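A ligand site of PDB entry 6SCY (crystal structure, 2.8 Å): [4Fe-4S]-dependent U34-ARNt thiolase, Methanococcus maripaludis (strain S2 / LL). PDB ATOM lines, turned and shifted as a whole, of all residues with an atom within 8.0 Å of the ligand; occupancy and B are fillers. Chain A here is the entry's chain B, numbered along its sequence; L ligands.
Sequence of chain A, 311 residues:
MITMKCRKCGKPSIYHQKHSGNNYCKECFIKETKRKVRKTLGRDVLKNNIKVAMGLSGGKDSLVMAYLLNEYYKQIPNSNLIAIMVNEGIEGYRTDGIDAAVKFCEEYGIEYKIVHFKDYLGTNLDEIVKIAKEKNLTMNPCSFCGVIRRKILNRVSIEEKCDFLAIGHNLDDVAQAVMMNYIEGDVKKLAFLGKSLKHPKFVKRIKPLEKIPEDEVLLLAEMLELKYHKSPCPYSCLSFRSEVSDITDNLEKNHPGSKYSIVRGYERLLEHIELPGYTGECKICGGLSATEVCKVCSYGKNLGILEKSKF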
ATOM      1  N   VAL A  86      11.826 -20.317  24.008  1.00  0.00           N
ATOM      2  CA  VAL A  86      13.129 -20.440  24.655  1.00  0.00           C
ATOM      3  C   VAL A  86      14.118 -19.445  24.061  1.00  0.00           C
ATOM      4  O   VAL A  86      14.652 -19.675  22.974  1.00  0.00           O
ATOM      5  CB  VAL A  86      13.655 -21.906  24.696  1.00  0.00           C
ATOM      6  CG1 VAL A  86      14.887 -22.035  25.587  1.00  0.00           C
ATOM      7  CG2 VAL A  86      12.566 -22.876  25.156  1.00  0.00           C
ATOM      8  N   GLU A  88      17.418 -18.030  23.439  1.00  0.00           N
ATOM      9  CA  GLU A  88      18.820 -18.447  23.422  1.00  0.00           C
ATOM     10  C   GLU A  88      19.745 -17.360  23.970  1.00  0.00           C
ATOM     11  O   GLU A  88      20.775 -17.676  24.551  1.00  0.00           O
ATOM     12  CB  GLU A  88      19.256 -18.862  22.021  1.00  0.00           C
ATOM     13  CG  GLU A  88      19.076 -20.333  21.724  1.00  0.00           C
ATOM     14  CD  GLU A  88      17.688 -20.762  21.282  1.00  0.00           C
ATOM     15  OE1 GLU A  88      17.363 -20.563  20.093  1.00  0.00           O
ATOM     16  OE2 GLU A  88      16.936 -21.310  22.121  1.00  0.00           O
ATOM     17  N   ILE A  90      21.047 -14.286  22.079  1.00  0.00           N
ATOM     18  CA  ILE A  90      22.093 -13.920  21.130  1.00  0.00           C
ATOM     19  C   ILE A  90      22.105 -12.388  20.948  1.00  0.00           C
ATOM     20  O   ILE A  90      21.033 -11.774  20.959  1.00  0.00           O
ATOM     21  CB  ILE A  90      21.966 -14.708  19.791  1.00  0.00           C
ATOM     22  CG1 ILE A  90      21.961 -16.246  20.051  1.00  0.00           C
ATOM     23  CG2 ILE A  90      23.064 -14.305  18.796  1.00  0.00           C
ATOM     24  CD1 ILE A  90      21.813 -17.193  18.827  1.00  0.00           C
ATOM     25  N   ARG A  94      17.299 -13.604  17.566  1.00  0.00           N
ATOM     26  CA  ARG A  94      16.546 -14.297  18.633  1.00  0.00           C
ATOM     27  C   ARG A  94      15.495 -13.408  19.321  1.00  0.00           C
ATOM     28  O   ARG A  94      14.395 -13.903  19.585  1.00  0.00           O
ATOM     29  CB  ARG A  94      17.457 -14.976  19.679  1.00  0.00           C
ATOM     30  CG  ARG A  94      18.341 -16.058  19.095  1.00  0.00           C
ATOM     31  CD  ARG A  94      17.697 -17.435  19.074  1.00  0.00           C
ATOM     32  NE  ARG A  94      17.140 -17.791  17.754  1.00  0.00           N
ATOM     33  CZ  ARG A  94      17.841 -18.336  16.766  1.00  0.00           C
ATOM     34  NH1 ARG A  94      19.137 -18.546  16.904  1.00  0.00           N
ATOM     35  NH2 ARG A  94      17.244 -18.646  15.621  1.00  0.00           N
ATOM     36  N   PHE A 117      17.717 -19.132  28.070  1.00  0.00           N
ATOM     37  CA  PHE A 117      18.861 -20.037  28.052  1.00  0.00           C
ATOM     38  C   PHE A 117      19.798 -19.634  29.187  1.00  0.00           C
ATOM     39  O   PHE A 117      20.339 -20.497  29.870  1.00  0.00           O
ATOM     40  CB  PHE A 117      19.594 -19.935  26.704  1.00  0.00           C
ATOM     41  CG  PHE A 117      19.671 -21.212  25.885  1.00  0.00           C
ATOM     42  CD1 PHE A 117      20.866 -21.915  25.785  1.00  0.00           C
ATOM     43  CD2 PHE A 117      18.566 -21.678  25.195  1.00  0.00           C
ATOM     44  CE1 PHE A 117      20.945 -23.081  25.034  1.00  0.00           C
ATOM     45  CE2 PHE A 117      18.647 -22.855  24.436  1.00  0.00           C
ATOM     46  CZ  PHE A 117      19.836 -23.543  24.360  1.00  0.00           C
ATOM     47  N   LEU A 125      25.278 -16.904  25.403  1.00  0.00           N
ATOM     48  CA  LEU A 125      25.780 -17.187  24.056  1.00  0.00           C
ATOM     49  C   LEU A 125      27.274 -17.587  24.004  1.00  0.00           C
ATOM     50  O   LEU A 125      28.137 -16.871  24.512  1.00  0.00           O
ATOM     51  CB  LEU A 125      25.483 -15.962  23.141  1.00  0.00           C
ATOM     52  CG  LEU A 125      25.720 -16.023  21.608  1.00  0.00           C
ATOM     53  CD1 LEU A 125      27.149 -15.638  21.254  1.00  0.00           C
ATOM     54  CD2 LEU A 125      25.314 -17.357  20.998  1.00  0.00           C
ATOM     55  N   ASP A 126      27.535 -18.738  23.341  1.00  0.00           N
ATOM     56  CA  ASP A 126      28.824 -19.370  23.034  1.00  0.00           C
ATOM     57  C   ASP A 126      29.747 -19.684  24.218  1.00  0.00           C
ATOM     58  O   ASP A 126      29.911 -18.900  25.146  1.00  0.00           O
ATOM     59  CB  ASP A 126      29.602 -18.580  21.976  1.00  0.00           C
ATOM     60  CG  ASP A 126      29.321 -19.067  20.570  1.00  0.00           C
ATOM     61  OD1 ASP A 126      28.171 -18.899  20.093  1.00  0.00           O
ATOM     62  OD2 ASP A 126      30.243 -19.619  19.936  1.00  0.00           O
ATOM     63  N   ASN A 140      30.640 -28.886  18.641  1.00  0.00           N
ATOM     64  CA  ASN A 140      29.562 -28.432  17.740  1.00  0.00           C
ATOM     65  C   ASN A 140      28.585 -27.426  18.376  1.00  0.00           C
ATOM     66  O   ASN A 140      28.073 -27.678  19.467  1.00  0.00           O
ATOM     67  CB  ASN A 140      28.821 -29.633  17.144  1.00  0.00           C
ATOM     68  CG  ASN A 140      29.611 -30.380  16.109  1.00  0.00           C
ATOM     69  OD1 ASN A 140      30.813 -30.634  16.258  1.00  0.00           O
ATOM     70  ND2 ASN A 140      28.941 -30.762  15.027  1.00  0.00           N
ATOM     71  N   PRO A 141      28.321 -26.284  17.687  1.00  0.00           N
ATOM     72  CA  PRO A 141      27.447 -25.235  18.258  1.00  0.00           C
ATOM     73  C   PRO A 141      25.941 -25.406  18.051  1.00  0.00           C
ATOM     74  O   PRO A 141      25.170 -25.226  19.002  1.00  0.00           O
ATOM     75  CB  PRO A 141      27.960 -23.933  17.588  1.00  0.00           C
ATOM     76  CG  PRO A 141      29.051 -24.367  16.624  1.00  0.00           C
ATOM     77  CD  PRO A 141      28.900 -25.833  16.407  1.00  0.00           C
ATOM     78  N   CYS A 142      25.524 -25.733  16.816  1.00  0.00           N
ATOM     79  CA  CYS A 142      24.113 -25.936  16.451  1.00  0.00           C
ATOM     80  C   CYS A 142      23.498 -27.151  17.161  1.00  0.00           C
ATOM     81  O   CYS A 142      22.331 -27.085  17.542  1.00  0.00           O
ATOM     82  CB  CYS A 142      23.960 -26.025  14.939  1.00  0.00           C
ATOM     83  SG  CYS A 142      22.262 -25.799  14.354  1.00  0.00           S
ATOM     84  N   SER A 143      24.286 -28.233  17.347  1.00  0.00           N
ATOM     85  CA  SER A 143      23.844 -29.457  18.012  1.00  0.00           C
ATOM     86  C   SER A 143      23.606 -29.213  19.511  1.00  0.00           C
ATOM     87  O   SER A 143      22.539 -29.561  20.020  1.00  0.00           O
ATOM     88  CB  SER A 143      24.851 -30.585  17.811  1.00  0.00           C
ATOM     89  OG  SER A 143      26.016 -30.426  18.613  1.00  0.00           O
ATOM     90  N   PHE A 144      24.597 -28.577  20.170  1.00  0.00           N
ATOM     91  CA  PHE A 144      24.620 -28.191  21.580  1.00  0.00           C
ATOM     92  C   PHE A 144      23.337 -27.442  21.948  1.00  0.00           C
ATOM     93  O   PHE A 144      22.693 -27.774  22.939  1.00  0.00           O
ATOM     94  CB  PHE A 144      25.887 -27.338  21.841  1.00  0.00           C
ATOM     95  CG  PHE A 144      25.976 -26.520  23.111  1.00  0.00           C
ATOM     96  CD1 PHE A 144      26.508 -27.067  24.277  1.00  0.00           C
ATOM     97  CD2 PHE A 144      25.633 -25.175  23.124  1.00  0.00           C
ATOM     98  CE1 PHE A 144      26.633 -26.294  25.440  1.00  0.00           C
ATOM     99  CE2 PHE A 144      25.743 -24.408  24.291  1.00  0.00           C
ATOM    100  CZ  PHE A 144      26.251 -24.975  25.431  1.00  0.00           C
ATOM    101  N   CYS A 145      22.954 -26.474  21.097  1.00  0.00           N
ATOM    102  CA  CYS A 145      21.769 -25.624  21.244  1.00  0.00           C
ATOM    103  C   CYS A 145      20.462 -26.411  21.190  1.00  0.00           C
ATOM    104  O   CYS A 145      19.599 -26.190  22.036  1.00  0.00           O
ATOM    105  CB  CYS A 145      21.795 -24.496  20.234  1.00  0.00           C
ATOM    106  SG  CYS A 145      20.340 -23.420  20.292  1.00  0.00           S
ATOM    107  N   GLY A 146      20.329 -27.277  20.188  1.00  0.00           N
ATOM    108  CA  GLY A 146      19.140 -28.110  19.999  1.00  0.00           C
ATOM    109  C   GLY A 146      18.914 -29.117  21.113  1.00  0.00           C
ATOM    110  O   GLY A 146      17.763 -29.343  21.508  1.00  0.00           O
ATOM    111  N   VAL A 147      20.022 -29.709  21.621  1.00  0.00           N
ATOM    112  CA  VAL A 147      20.018 -30.705  22.711  1.00  0.00           C
ATOM    113  C   VAL A 147      19.531 -30.083  24.026  1.00  0.00           C
ATOM    114  O   VAL A 147      18.634 -30.640  24.673  1.00  0.00           O
ATOM    115  CB  VAL A 147      21.388 -31.444  22.842  1.00  0.00           C
ATOM    116  CG1 VAL A 147      21.459 -32.295  24.109  1.00  0.00           C
ATOM    117  CG2 VAL A 147      21.666 -32.308  21.616  1.00  0.00           C
ATOM    118  N   ARG A 149      17.827 -27.087  24.403  1.00  0.00           N
ATOM    119  CA  ARG A 149      16.458 -26.623  24.160  1.00  0.00           C
ATOM    120  C   ARG A 149      15.432 -27.722  24.476  1.00  0.00           C
ATOM    121  O   ARG A 149      14.428 -27.452  25.127  1.00  0.00           O
ATOM    122  CB  ARG A 149      16.320 -26.127  22.717  1.00  0.00           C
ATOM    123  CG  ARG A 149      15.021 -25.390  22.364  1.00  0.00           C
ATOM    124  CD  ARG A 149      15.112 -24.600  21.059  1.00  0.00           C
ATOM    125  NE  ARG A 149      15.359 -25.445  19.893  1.00  0.00           N
ATOM    126  CZ  ARG A 149      16.535 -25.549  19.265  1.00  0.00           C
ATOM    127  NH1 ARG A 149      17.582 -24.863  19.689  1.00  0.00           N
ATOM    128  NH2 ARG A 149      16.658 -26.346  18.207  1.00  0.00           N
ATOM    129  N   SER A 231      13.264 -15.311  11.677  1.00  0.00           N
ATOM    130  CA  SER A 231      14.338 -15.216  12.678  1.00  0.00           C
ATOM    131  C   SER A 231      15.600 -16.039  12.295  1.00  0.00           C
ATOM    132  O   SER A 231      15.806 -17.144  12.834  1.00  0.00           O
ATOM    133  CB  SER A 231      13.842 -15.512  14.090  1.00  0.00           C
ATOM    134  OG  SER A 231      13.523 -16.878  14.296  1.00  0.00           O
ATOM    135  N   PRO A 232      16.437 -15.527  11.359  1.00  0.00           N
ATOM    136  CA  PRO A 232      17.645 -16.283  10.973  1.00  0.00           C
ATOM    137  C   PRO A 232      18.711 -16.295  12.084  1.00  0.00           C
ATOM    138  O   PRO A 232      18.935 -15.265  12.726  1.00  0.00           O
ATOM    139  CB  PRO A 232      18.140 -15.559   9.709  1.00  0.00           C
ATOM    140  CG  PRO A 232      17.057 -14.585   9.345  1.00  0.00           C
ATOM    141  CD  PRO A 232      16.357 -14.260  10.621  1.00  0.00           C
ATOM    142  N   CYS A 233      19.327 -17.466  12.311  1.00  0.00           N
ATOM    143  CA  CYS A 233      20.342 -17.685  13.350  1.00  0.00           C
ATOM    144  C   CYS A 233      21.684 -16.985  13.030  1.00  0.00           C
ATOM    145  O   CYS A 233      22.299 -17.304  12.003  1.00  0.00           O
ATOM    146  CB  CYS A 233      20.540 -19.169  13.631  1.00  0.00           C
ATOM    147  SG  CYS A 233      21.568 -19.525  15.086  1.00  0.00           S
ATOM    148  N   PRO A 234      22.165 -16.045  13.886  1.00  0.00           N
ATOM    149  CA  PRO A 234      23.437 -15.369  13.603  1.00  0.00           C
ATOM    150  C   PRO A 234      24.696 -16.140  14.037  1.00  0.00           C
ATOM    151  O   PRO A 234      25.803 -15.689  13.738  1.00  0.00           O
ATOM    152  CB  PRO A 234      23.314 -14.032  14.336  1.00  0.00           C
ATOM    153  CG  PRO A 234      22.135 -14.170  15.258  1.00  0.00           C
ATOM    154  CD  PRO A 234      21.571 -15.554  15.136  1.00  0.00           C
ATOM    155  N   TYR A 235      24.535 -17.306  14.712  1.00  0.00           N
ATOM    156  CA  TYR A 235      25.672 -18.099  15.180  1.00  0.00           C
ATOM    157  C   TYR A 235      25.669 -19.568  14.701  1.00  0.00           C
ATOM    158  O   TYR A 235      26.532 -20.329  15.130  1.00  0.00           O
ATOM    159  CB  TYR A 235      25.805 -18.010  16.712  1.00  0.00           C
ATOM    160  CG  TYR A 235      26.637 -16.845  17.187  1.00  0.00           C
ATOM    161  CD1 TYR A 235      28.003 -16.990  17.430  1.00  0.00           C
ATOM    162  CD2 TYR A 235      26.079 -15.580  17.371  1.00  0.00           C
ATOM    163  CE1 TYR A 235      28.785 -15.906  17.860  1.00  0.00           C
ATOM    164  CE2 TYR A 235      26.847 -14.495  17.796  1.00  0.00           C
ATOM    165  CZ  TYR A 235      28.207 -14.663  18.031  1.00  0.00           C
ATOM    166  OH  TYR A 235      28.972 -13.602  18.463  1.00  0.00           O
ATOM    167  N   SER A 236      24.740 -19.947  13.778  1.00  0.00           N
ATOM    168  CA  SER A 236      24.678 -21.308  13.220  1.00  0.00           C
ATOM    169  C   SER A 236      24.057 -21.395  11.823  1.00  0.00           C
ATOM    170  O   SER A 236      22.955 -20.889  11.583  1.00  0.00           O
ATOM    171  CB  SER A 236      23.966 -22.272  14.165  1.00  0.00           C
ATOM    172  OG  SER A 236      24.817 -22.695  15.219  1.00  0.00           O
ATOM    173  N   CYS A 237      24.770 -22.075  10.915  1.00  0.00           N
ATOM    174  CA  CYS A 237      24.386 -22.291   9.514  1.00  0.00           C
ATOM    175  C   CYS A 237      24.974 -23.631   9.031  1.00  0.00           C
ATOM    176  O   CYS A 237      26.147 -23.696   8.627  1.00  0.00           O
ATOM    177  CB  CYS A 237      24.833 -21.126   8.637  1.00  0.00           C
ATOM    178  SG  CYS A 237      24.585 -21.382   6.855  1.00  0.00           S
ATOM    179  N   LEU A 238      24.155 -24.695   9.095  1.00  0.00           N
ATOM    180  CA  LEU A 238      24.574 -26.014   8.642  1.00  0.00           C
ATOM    181  C   LEU A 238      24.090 -26.171   7.191  1.00  0.00           C
ATOM    182  O   LEU A 238      22.893 -26.197   6.913  1.00  0.00           O
ATOM    183  CB  LEU A 238      24.072 -27.114   9.597  1.00  0.00           C
ATOM    184  CG  LEU A 238      24.760 -28.500   9.502  1.00  0.00           C
ATOM    185  CD1 LEU A 238      25.335 -28.979  10.890  1.00  0.00           C
ATOM    186  CD2 LEU A 238      23.767 -29.491   8.877  1.00  0.00           C
HETATM  187 FE1  LIG L   1      21.484 -24.126  15.775  1.00  0.00          FE
HETATM  188 FE2  LIG L   1      20.408 -23.230  18.143  1.00  0.00          FE
HETATM  189 FE3  LIG L   1      18.835 -23.364  15.895  1.00  0.00          FE
HETATM  190 FE4  LIG L   1      20.819 -21.471  16.078  1.00  0.00          FE
HETATM  191  S1  LIG L   1      18.943 -21.632  17.395  1.00  0.00           S
HETATM  192  S2  LIG L   1      20.356 -22.805  14.254  1.00  0.00           S
HETATM  193  S3  LIG L   1      22.436 -22.631  17.236  1.00  0.00           S
HETATM  194  S4  LIG L   1      19.810 -25.140  17.004  1.00  0.00           S
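The side-chain sulfur (SG) of Cys 145 binds an iron atom (FE2) of the ligand, at 2.2 Å. SG of Cys 233 is bound to FE4 of the ligand, 2.3 Å away. SG of Cys 142 binds FE1 of the ligand, at 2.3 Å. S3 of the ligand lies close to OG of Ser 236 (3.1 Å). S1 of the ligand sits close to NH1 of Arg 94, 3.1 Å away. The guanidinium group (NH1) of Arg 149 lies close to a sulfur (S4) of the ligand, 3.5 Å away.
NH1 of Arg 149 sits close to O of Cys 145 (3.4 Å). The side-chain sulfur (SG) of Cys 233 lies close to the backbone NH (N) of Ser 236. The side-chain sulfur (SG) of Cys 233 lies close to the guanidinium group (NH1) of Arg 94, 3.2 Å away. The side-chain sulfur of Cys 233 lies close to the backbone NH of Tyr 235, at 3.7 Å. The guanidinium group (NE) of Arg 94 is in salt-bridge range of the side-chain carboxylate (OE1) of Glu 88. The backbone carbonyl oxygen (O) of Ser 231 lies within hydrogen-bond range of the guanidinium group (NH2) of Arg 94, 3.5 Å away.
S1 of the ligand lies close to OE1 of Glu 88, at 3.3 Å. Residues that only touch the ligand: Gly 146 (3.9 Å). Eight residues have an atom within 4 Å of the ligand: Glu 88, Arg 94, Cys 142, Cys 145, Gly 146, Arg 149, Cys 233 and Ser 236. The nearest printed residue that does not touch the ligand is Pro 141 (4.2 Å).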
